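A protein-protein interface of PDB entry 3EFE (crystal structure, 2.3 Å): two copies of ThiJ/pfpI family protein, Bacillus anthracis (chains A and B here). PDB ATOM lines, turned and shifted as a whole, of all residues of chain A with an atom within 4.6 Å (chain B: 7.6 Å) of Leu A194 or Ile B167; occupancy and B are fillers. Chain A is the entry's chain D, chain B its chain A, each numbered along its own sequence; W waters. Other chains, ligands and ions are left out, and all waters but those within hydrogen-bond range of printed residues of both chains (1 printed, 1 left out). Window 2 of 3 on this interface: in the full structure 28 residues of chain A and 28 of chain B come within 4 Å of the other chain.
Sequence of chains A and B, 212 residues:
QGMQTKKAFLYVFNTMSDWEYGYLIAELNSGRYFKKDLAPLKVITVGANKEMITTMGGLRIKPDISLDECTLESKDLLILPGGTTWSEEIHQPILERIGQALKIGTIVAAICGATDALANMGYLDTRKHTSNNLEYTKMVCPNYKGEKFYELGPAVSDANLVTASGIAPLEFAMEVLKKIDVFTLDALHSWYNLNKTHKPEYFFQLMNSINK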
ATOM      1  N   SER A 190      16.686  10.398  18.726  1.00  0.00           N
ATOM      2  CA  SER A 190      16.320  10.394  17.330  1.00  0.00           C
ATOM      3  C   SER A 190      17.333  11.172  16.451  1.00  0.00           C
ATOM      4  O   SER A 190      17.604  10.765  15.317  1.00  0.00           O
ATOM      5  CB  SER A 190      14.900  10.957  17.189  1.00  0.00           C
ATOM      6  OG  SER A 190      14.853  12.277  17.708  1.00  0.00           O
ATOM      7  N   TRP A 191      17.854  12.285  16.978  1.00  0.00           N
ATOM      8  CA  TRP A 191      18.927  13.055  16.347  1.00  0.00           C
ATOM      9  C   TRP A 191      20.182  12.147  16.187  1.00  0.00           C
ATOM     10  O   TRP A 191      20.738  11.994  15.131  1.00  0.00           O
ATOM     11  CB  TRP A 191      19.286  14.286  17.183  1.00  0.00           C
ATOM     12  CG  TRP A 191      20.405  15.042  16.621  1.00  0.00           C
ATOM     13  CD1 TRP A 191      20.346  15.934  15.602  1.00  0.00           C
ATOM     14  CD2 TRP A 191      21.795  14.963  16.980  1.00  0.00           C
ATOM     15  NE1 TRP A 191      21.578  16.414  15.302  1.00  0.00           N
ATOM     16  CE2 TRP A 191      22.489  15.865  16.149  1.00  0.00           C
ATOM     17  CE3 TRP A 191      22.520  14.218  17.917  1.00  0.00           C
ATOM     18  CZ2 TRP A 191      23.881  16.044  16.223  1.00  0.00           C
ATOM     19  CZ3 TRP A 191      23.875  14.408  17.997  1.00  0.00           C
ATOM     20  CH2 TRP A 191      24.547  15.308  17.166  1.00  0.00           C
ATOM     21  N   TYR A 192      20.562  11.492  17.261  1.00  0.00           N
ATOM     22  CA  TYR A 192      21.692  10.585  17.248  1.00  0.00           C
ATOM     23  C   TYR A 192      21.456   9.494  16.254  1.00  0.00           C
ATOM     24  O   TYR A 192      22.302   9.219  15.435  1.00  0.00           O
ATOM     25  CB  TYR A 192      21.941   9.957  18.621  1.00  0.00           C
ATOM     26  CG  TYR A 192      23.083   8.962  18.559  1.00  0.00           C
ATOM     27  CD1 TYR A 192      24.377   9.381  18.271  1.00  0.00           C
ATOM     28  CD2 TYR A 192      22.852   7.591  18.709  1.00  0.00           C
ATOM     29  CE1 TYR A 192      25.403   8.474  18.177  1.00  0.00           C
ATOM     30  CE2 TYR A 192      23.891   6.675  18.611  1.00  0.00           C
ATOM     31  CZ  TYR A 192      25.144   7.121  18.345  1.00  0.00           C
ATOM     32  OH  TYR A 192      26.153   6.215  18.301  1.00  0.00           O
ATOM     33  N   ASN A 193      20.303   8.863  16.322  1.00  0.00           N
ATOM     34  CA  ASN A 193      19.990   7.732  15.420  1.00  0.00           C
ATOM     35  C   ASN A 193      19.882   8.076  13.957  1.00  0.00           C
ATOM     36  O   ASN A 193      20.244   7.265  13.129  1.00  0.00           O
ATOM     37  CB  ASN A 193      18.716   6.990  15.846  1.00  0.00           C
ATOM     38  CG  ASN A 193      18.882   6.150  17.118  1.00  0.00           C
ATOM     39  OD1 ASN A 193      19.956   5.695  17.472  1.00  0.00           O
ATOM     40  ND2 ASN A 193      17.768   5.913  17.781  1.00  0.00           N
ATOM     41  N   LEU A 194      19.364   9.252  13.634  1.00  0.00           N
ATOM     42  CA  LEU A 194      19.237   9.716  12.236  1.00  0.00           C
ATOM     43  C   LEU A 194      20.643   9.888  11.636  1.00  0.00           C
ATOM     44  O   LEU A 194      20.954   9.365  10.576  1.00  0.00           O
ATOM     45  CB  LEU A 194      18.467  11.037  12.161  1.00  0.00           C
ATOM     46  CG  LEU A 194      18.365  11.755  10.817  1.00  0.00           C
ATOM     47  CD1 LEU A 194      17.575  10.931   9.791  1.00  0.00           C
ATOM     48  CD2 LEU A 194      17.833  13.198  11.009  1.00  0.00           C
ATOM     49  N   ASN A 195      21.481  10.627  12.343  1.00  0.00           N
ATOM     50  CA  ASN A 195      22.815  10.870  11.904  1.00  0.00           C
ATOM     51  C   ASN A 195      23.661   9.591  11.792  1.00  0.00           C
ATOM     52  O   ASN A 195      24.403   9.440  10.863  1.00  0.00           O
ATOM     53  CB  ASN A 195      23.471  11.934  12.814  1.00  0.00           C
ATOM     54  CG  ASN A 195      22.991  13.335  12.513  1.00  0.00           C
ATOM     55  OD1 ASN A 195      23.458  13.939  11.572  1.00  0.00           O
ATOM     56  ND2 ASN A 195      22.060  13.854  13.293  1.00  0.00           N
ATOM     57  N   LYS A 196      23.520   8.666  12.722  1.00  0.00           N
ATOM     58  CA  LYS A 196      24.279   7.421  12.773  1.00  0.00           C
ATOM     59  C   LYS A 196      23.808   6.410  11.702  1.00  0.00           C
ATOM     60  O   LYS A 196      24.581   5.785  10.974  1.00  0.00           O
ATOM     61  CB  LYS A 196      24.110   6.828  14.157  1.00  0.00           C
ATOM     62  CG  LYS A 196      25.102   5.698  14.552  1.00  0.00           C
ATOM     63  CD  LYS A 196      26.572   6.217  14.687  1.00  0.00           C
ATOM     64  CE  LYS A 196      27.500   5.116  15.082  1.00  0.00           C
ATOM     65  NZ  LYS A 196      28.947   5.557  15.099  1.00  0.00           N
ATOM     66  N   THR A 197      22.508   6.289  11.589  1.00  0.00           N
ATOM     67  CA  THR A 197      21.815   5.195  10.891  1.00  0.00           C
ATOM     68  C   THR A 197      21.283   5.613   9.539  1.00  0.00           C
ATOM     69  O   THR A 197      21.073   4.783   8.682  1.00  0.00           O
ATOM     70  CB  THR A 197      20.683   4.773  11.888  1.00  0.00           C
ATOM     71  OG1 THR A 197      21.220   3.799  12.817  1.00  0.00           O
ATOM     72  CG2 THR A 197      19.410   4.374  11.259  1.00  0.00           C
ATOM     73  N   HIS A 198      21.033   6.912   9.382  1.00  0.00           N
ATOM     74  CA  HIS A 198      20.326   7.536   8.227  1.00  0.00           C
ATOM     75  C   HIS A 198      18.942   7.010   7.955  1.00  0.00           C
ATOM     76  O   HIS A 198      18.463   7.192   6.863  1.00  0.00           O
ATOM     77  CB  HIS A 198      21.118   7.471   6.917  1.00  0.00           C
ATOM     78  CG  HIS A 198      22.566   7.777   7.078  1.00  0.00           C
ATOM     79  ND1 HIS A 198      23.030   8.671   8.014  1.00  0.00           N
ATOM     80  CD2 HIS A 198      23.650   7.296   6.435  1.00  0.00           C
ATOM     81  CE1 HIS A 198      24.337   8.714   7.965  1.00  0.00           C
ATOM     82  NE2 HIS A 198      24.742   7.859   7.040  1.00  0.00           N
ATOM     83  N   LYS A 199      18.310   6.344   8.923  1.00  0.00           N
ATOM     84  CA  LYS A 199      16.997   5.746   8.674  1.00  0.00           C
ATOM     85  C   LYS A 199      15.978   6.859   8.853  1.00  0.00           C
ATOM     86  O   LYS A 199      16.078   7.641   9.762  1.00  0.00           O
ATOM     87  CB  LYS A 199      16.701   4.546   9.592  1.00  0.00           C
ATOM     88  CG  LYS A 199      17.554   3.361   9.304  1.00  0.00           C
ATOM     89  CD  LYS A 199      17.117   2.067   9.973  1.00  0.00           C
ATOM     90  CE  LYS A 199      15.931   1.402   9.174  1.00  0.00           C
ATOM     91  NZ  LYS A 199      14.745   0.926  10.113  1.00  0.00           N
ATOM     92  N   TYR A 202      13.629   8.264  11.882  1.00  0.00           N
ATOM     93  CA  TYR A 202      14.272   9.109  12.899  1.00  0.00           C
ATOM     94  C   TYR A 202      14.176  10.581  12.548  1.00  0.00           C
ATOM     95  O   TYR A 202      14.257  11.425  13.409  1.00  0.00           O
ATOM     96  CB  TYR A 202      15.731   8.721  13.072  1.00  0.00           C
ATOM     97  CG  TYR A 202      15.906   7.340  13.593  1.00  0.00           C
ATOM     98  CD1 TYR A 202      15.424   7.017  14.847  1.00  0.00           C
ATOM     99  CD2 TYR A 202      16.566   6.362  12.855  1.00  0.00           C
ATOM    100  CE1 TYR A 202      15.571   5.750  15.375  1.00  0.00           C
ATOM    101  CE2 TYR A 202      16.722   5.065  13.359  1.00  0.00           C
ATOM    102  CZ  TYR A 202      16.215   4.756  14.633  1.00  0.00           C
ATOM    103  OH  TYR A 202      16.317   3.500  15.200  1.00  0.00           O
ATOM    104  N   PHE A 203      14.023  10.879  11.275  1.00  0.00           N
ATOM    105  CA  PHE A 203      13.808  12.245  10.854  1.00  0.00           C
ATOM    106  C   PHE A 203      12.371  12.655  11.298  1.00  0.00           C
ATOM    107  O   PHE A 203      12.167  13.710  11.914  1.00  0.00           O
ATOM    108  CB  PHE A 203      14.060  12.404   9.327  1.00  0.00           C
ATOM    109  CG  PHE A 203      13.521  13.683   8.792  1.00  0.00           C
ATOM    110  CD1 PHE A 203      14.258  14.870   8.944  1.00  0.00           C
ATOM    111  CD2 PHE A 203      12.229  13.740   8.266  1.00  0.00           C
ATOM    112  CE1 PHE A 203      13.733  16.044   8.507  1.00  0.00           C
ATOM    113  CE2 PHE A 203      11.708  14.895   7.828  1.00  0.00           C
ATOM    114  CZ  PHE A 203      12.434  16.061   7.975  1.00  0.00           C
ATOM    115  N   LEU A 206      12.385  13.039  15.120  1.00  0.00           N
ATOM    116  CA  LEU A 206      13.103  14.236  15.492  1.00  0.00           C
ATOM    117  C   LEU A 206      12.302  15.485  15.256  1.00  0.00           C
ATOM    118  O   LEU A 206      12.294  16.314  16.109  1.00  0.00           O
ATOM    119  CB  LEU A 206      14.452  14.296  14.733  1.00  0.00           C
ATOM    120  CG  LEU A 206      15.268  15.581  14.948  1.00  0.00           C
ATOM    121  CD1 LEU A 206      15.643  15.759  16.417  1.00  0.00           C
ATOM    122  CD2 LEU A 206      16.515  15.651  14.088  1.00  0.00           C
ATOM    123  N   TRP B  19      29.488  20.422   9.963  1.00  0.00           N
ATOM    124  CA  TRP B  19      29.740  18.985  10.010  1.00  0.00           C
ATOM    125  C   TRP B  19      29.779  18.297   8.616  1.00  0.00           C
ATOM    126  O   TRP B  19      30.098  17.123   8.493  1.00  0.00           O
ATOM    127  CB  TRP B  19      28.618  18.377  10.859  1.00  0.00           C
ATOM    128  CG  TRP B  19      27.325  18.339  10.186  1.00  0.00           C
ATOM    129  CD1 TRP B  19      26.880  17.350   9.355  1.00  0.00           C
ATOM    130  CD2 TRP B  19      26.291  19.304  10.253  1.00  0.00           C
ATOM    131  NE1 TRP B  19      25.630  17.645   8.906  1.00  0.00           N
ATOM    132  CE2 TRP B  19      25.235  18.836   9.445  1.00  0.00           C
ATOM    133  CE3 TRP B  19      26.122  20.509  10.954  1.00  0.00           C
ATOM    134  CZ2 TRP B  19      24.018  19.528   9.314  1.00  0.00           C
ATOM    135  CZ3 TRP B  19      24.937  21.182  10.822  1.00  0.00           C
ATOM    136  CH2 TRP B  19      23.902  20.708   9.984  1.00  0.00           C
ATOM    137  N   GLU B  20      29.351  19.022   7.590  1.00  0.00           N
ATOM    138  CA  GLU B  20      29.079  18.418   6.317  1.00  0.00           C
ATOM    139  C   GLU B  20      30.333  18.276   5.444  1.00  0.00           C
ATOM    140  O   GLU B  20      30.392  17.358   4.700  1.00  0.00           O
ATOM    141  CB  GLU B  20      27.974  19.209   5.598  1.00  0.00           C
ATOM    142  CG  GLU B  20      26.587  18.977   6.212  1.00  0.00           C
ATOM    143  CD  GLU B  20      25.498  19.678   5.469  1.00  0.00           C
ATOM    144  OE1 GLU B  20      25.814  20.398   4.470  1.00  0.00           O
ATOM    145  OE2 GLU B  20      24.318  19.553   5.926  1.00  0.00           O
ATOM    146  N   ILE B 111      26.326  18.870  -1.028  1.00  0.00           N
ATOM    147  CA  ILE B 111      25.754  18.170   0.095  1.00  0.00           C
ATOM    148  C   ILE B 111      24.572  19.000   0.627  1.00  0.00           C
ATOM    149  O   ILE B 111      24.617  20.251   0.634  1.00  0.00           O
ATOM    150  CB  ILE B 111      26.832  17.818   1.202  1.00  0.00           C
ATOM    151  CG1 ILE B 111      26.187  17.087   2.408  1.00  0.00           C
ATOM    152  CG2 ILE B 111      27.607  19.024   1.610  1.00  0.00           C
ATOM    153  CD1 ILE B 111      27.025  16.016   3.029  1.00  0.00           C
ATOM    154  N   CYS B 112      23.510  18.297   1.011  1.00  0.00           N
ATOM    155  CA  CYS B 112      22.419  18.894   1.763  1.00  0.00           C
ATOM    156  C   CYS B 112      21.648  19.951   0.901  1.00  0.00           C
ATOM    157  O   CYS B 112      21.290  19.672  -0.257  1.00  0.00           O
ATOM    158  CB  CYS B 112      22.993  19.451   3.080  1.00  0.00           C
ATOM    159  SG  CYS B 112      21.740  19.782   4.450  1.00  0.00           S
ATOM    160  N   SER B 131      19.341  13.848  -2.377  1.00  0.00           N
ATOM    161  CA  SER B 131      19.125  15.091  -1.660  1.00  0.00           C
ATOM    162  C   SER B 131      18.744  14.672  -0.262  1.00  0.00           C
ATOM    163  O   SER B 131      18.802  13.469   0.067  1.00  0.00           O
ATOM    164  CB  SER B 131      18.003  15.891  -2.303  1.00  0.00           C
ATOM    165  OG  SER B 131      16.732  15.412  -1.875  1.00  0.00           O
ATOM    166  N   ASN B 132      18.345  15.634   0.574  1.00  0.00           N
ATOM    167  CA  ASN B 132      17.908  15.248   1.921  1.00  0.00           C
ATOM    168  C   ASN B 132      16.625  14.381   1.896  1.00  0.00           C
ATOM    169  O   ASN B 132      16.523  13.376   2.629  1.00  0.00           O
ATOM    170  CB  ASN B 132      17.792  16.477   2.832  1.00  0.00           C
ATOM    171  CG  ASN B 132      19.156  17.061   3.174  1.00  0.00           C
ATOM    172  OD1 ASN B 132      20.177  16.347   3.212  1.00  0.00           O
ATOM    173  ND2 ASN B 132      19.198  18.355   3.385  1.00  0.00           N
ATOM    174  N   PRO B 154      22.596   7.440   0.665  1.00  0.00           N
ATOM    175  CA  PRO B 154      22.623   8.918   0.876  1.00  0.00           C
ATOM    176  C   PRO B 154      23.772   9.691   0.212  1.00  0.00           C
ATOM    177  O   PRO B 154      23.866  10.897   0.381  1.00  0.00           O
ATOM    178  CB  PRO B 154      22.790   9.022   2.395  1.00  0.00           C
ATOM    179  CG  PRO B 154      23.707   7.885   2.706  1.00  0.00           C
ATOM    180  CD  PRO B 154      23.177   6.749   1.839  1.00  0.00           C
ATOM    181  N   ALA B 164      25.044  14.461  -1.814  1.00  0.00           N
ATOM    182  CA  ALA B 164      24.682  13.725  -0.629  1.00  0.00           C
ATOM    183  C   ALA B 164      23.647  14.450   0.213  1.00  0.00           C
ATOM    184  O   ALA B 164      23.471  15.650   0.103  1.00  0.00           O
ATOM    185  CB  ALA B 164      25.950  13.384   0.236  1.00  0.00           C
ATOM    186  N   SER B 165      22.958  13.696   1.060  1.00  0.00           N
ATOM    187  CA  SER B 165      22.234  14.258   2.162  1.00  0.00           C
ATOM    188  C   SER B 165      23.150  14.737   3.341  1.00  0.00           C
ATOM    189  O   SER B 165      24.210  14.137   3.614  1.00  0.00           O
ATOM    190  CB  SER B 165      21.212  13.263   2.646  1.00  0.00           C
ATOM    191  OG  SER B 165      21.888  12.239   3.230  1.00  0.00           O
ATOM    192  N   GLY B 166      22.739  15.785   4.054  1.00  0.00           N
ATOM    193  CA  GLY B 166      23.590  16.422   5.066  1.00  0.00           C
ATOM    194  C   GLY B 166      23.924  15.532   6.237  1.00  0.00           C
ATOM    195  O   GLY B 166      24.881  15.739   6.935  1.00  0.00           O
ATOM    196  N   ILE B 167      23.121  14.503   6.362  1.00  0.00           N
ATOM    197  CA  ILE B 167      23.093  13.515   7.386  1.00  0.00           C
ATOM    198  C   ILE B 167      24.274  12.510   7.175  1.00  0.00           C
ATOM    199  O   ILE B 167      24.650  11.746   8.109  1.00  0.00           O
ATOM    200  CB  ILE B 167      21.728  12.889   7.116  1.00  0.00           C
ATOM    201  CG1 ILE B 167      20.954  12.311   8.229  1.00  0.00           C
ATOM    202  CG2 ILE B 167      21.813  11.666   6.327  1.00  0.00           C
ATOM    203  CD1 ILE B 167      19.956  11.286   7.449  1.00  0.00           C
ATOM    204  N   ALA B 168      24.874  12.522   5.959  1.00  0.00           N
ATOM    205  CA  ALA B 168      25.899  11.567   5.529  1.00  0.00           C
ATOM    206  C   ALA B 168      27.243  12.170   5.107  1.00  0.00           C
ATOM    207  O   ALA B 168      27.753  11.828   4.014  1.00  0.00           O
ATOM    208  CB  ALA B 168      25.383  10.784   4.348  1.00  0.00           C
ATOM    209  N   PRO B 169      27.865  13.014   5.931  1.00  0.00           N
ATOM    210  CA  PRO B 169      29.186  13.566   5.574  1.00  0.00           C
ATOM    211  C   PRO B 169      30.336  12.579   5.305  1.00  0.00           C
ATOM    212  O   PRO B 169      31.274  12.938   4.622  1.00  0.00           O
ATOM    213  CB  PRO B 169      29.551  14.406   6.785  1.00  0.00           C
ATOM    214  CG  PRO B 169      28.707  13.905   7.855  1.00  0.00           C
ATOM    215  CD  PRO B 169      27.462  13.433   7.257  1.00  0.00           C
ATOM    216  N   LEU B 170      30.266  11.375   5.871  1.00  0.00           N
ATOM    217  CA  LEU B 170      31.286  10.344   5.746  1.00  0.00           C
ATOM    218  C   LEU B 170      31.229   9.677   4.392  1.00  0.00           C
ATOM    219  O   LEU B 170      32.240   9.558   3.762  1.00  0.00           O
ATOM    220  CB  LEU B 170      31.088   9.264   6.788  1.00  0.00           C
ATOM    221  CG  LEU B 170      31.854   9.439   8.129  1.00  0.00           C
ATOM    222  CD1 LEU B 170      31.643   8.232   9.021  1.00  0.00           C
ATOM    223  CD2 LEU B 170      33.326   9.661   7.885  1.00  0.00           C
ATOM    224  N   GLU B 171      30.020   9.306   3.965  1.00  0.00           N
ATOM    225  CA  GLU B 171      29.705   8.785   2.656  1.00  0.00           C
ATOM    226  C   GLU B 171      29.997   9.809   1.530  1.00  0.00           C
ATOM    227  O   GLU B 171      30.475   9.440   0.450  1.00  0.00           O
ATOM    228  CB  GLU B 171      28.228   8.388   2.597  1.00  0.00           C
ATOM    229  CG  GLU B 171      27.847   7.151   3.376  1.00  0.00           C
ATOM    230  CD  GLU B 171      27.674   7.354   4.912  1.00  0.00           C
ATOM    231  OE1 GLU B 171      27.624   8.508   5.432  1.00  0.00           O
ATOM    232  OE2 GLU B 171      27.639   6.325   5.625  1.00  0.00           O
ATOM    233  N   LYS B 196      32.851   4.959  10.447  1.00  0.00           N
ATOM    234  CA  LYS B 196      31.509   4.405  10.663  1.00  0.00           C
ATOM    235  C   LYS B 196      31.304   3.506  11.872  1.00  0.00           C
ATOM    236  O   LYS B 196      30.230   3.432  12.462  1.00  0.00           O
ATOM    237  CB  LYS B 196      31.064   3.583   9.449  1.00  0.00           C
ATOM    238  CG  LYS B 196      30.569   4.438   8.320  1.00  0.00           C
ATOM    239  CD  LYS B 196      29.269   5.239   8.618  1.00  0.00           C
ATOM    240  CE  LYS B 196      28.004   4.424   8.286  1.00  0.00           C
ATOM    241  NZ  LYS B 196      26.708   5.216   8.410  1.00  0.00           N
HETATM  242  O   HOH W   1      25.587  12.700  10.309  1.00  0.00           O
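O of Ile B167 sits close to ND1 of His A198 (3.5 Å). The side-chain carboxylate of Glu B171 lies within hydrogen-bond range of a ring nitrogen (NE2) of His A198, at 3.4 Å. O of Lys A196 is in hydrogen-bond range of NZ of Lys B196 (3.4 Å).
The backbone carbonyl oxygen (O) of Pro B154 sits at hydrogen-bond distance from the backbone NH (N) of Ser B165, 3.0 Å away. NZ of Lys B196 is in salt-bridge range of OE2 of Glu B171 (3.1 Å). ND2 of Asn A195 sits at hydrogen-bond distance from O of Trp A191, 2.9 Å away. O of Leu A194 lies close to ND1 of His A198, 3.4 Å away. The backbone carbonyl oxygen of Asn A195 lies close to a ring nitrogen (ND1) of His A198 (3.3 Å).
Among the printed residues, merely in contact across the chains: Leu A194 with Ile B167, His A198 with Lys B196, Asn A195 with Ile B167 and His A198 with Pro B154.
Of chain B, only Ile B167 (3.4 Å) comes within 4 Å of Leu A194. Ile B167 touches just these residues of chain A: Leu A194, Asn A195 and His A198. Of the printed residues of chain A, Lys B196 touches Lys A196 and His A198. Of the printed residues of chain B, His A198 touches Pro B154 (3.8 Å), Ile B167 (3.1 Å), Glu B171 (3.4 Å) and Lys B196 (3.6 Å). The nearest residue of chain B that does not touch Leu A194 is Ala B168 (6.8 Å). The nearest printed residue of chain B that does not touch Lys A196 is Ile B167 (5.7 Å).
Hydrophobic or aromatic side chains of chain B that line the printed part of chain A: Pro B154 and Ile B167. Along chain B the printed residues that touch a printed residue of chain A span positions 154 to 196. Among the printed residues, 7 pairs touch across the chains.
Lys A196 touches its own counterpart, Lys B196. Position printed for both chains: 196. Of the 7 pairs that touch across the chains among the printed residues, 1 has its exchanged pair printed and touching as well.
Water W1 bridges O of Ile B167 (2.6 Å) and OD1 of Asn A195 (2.8 Å).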
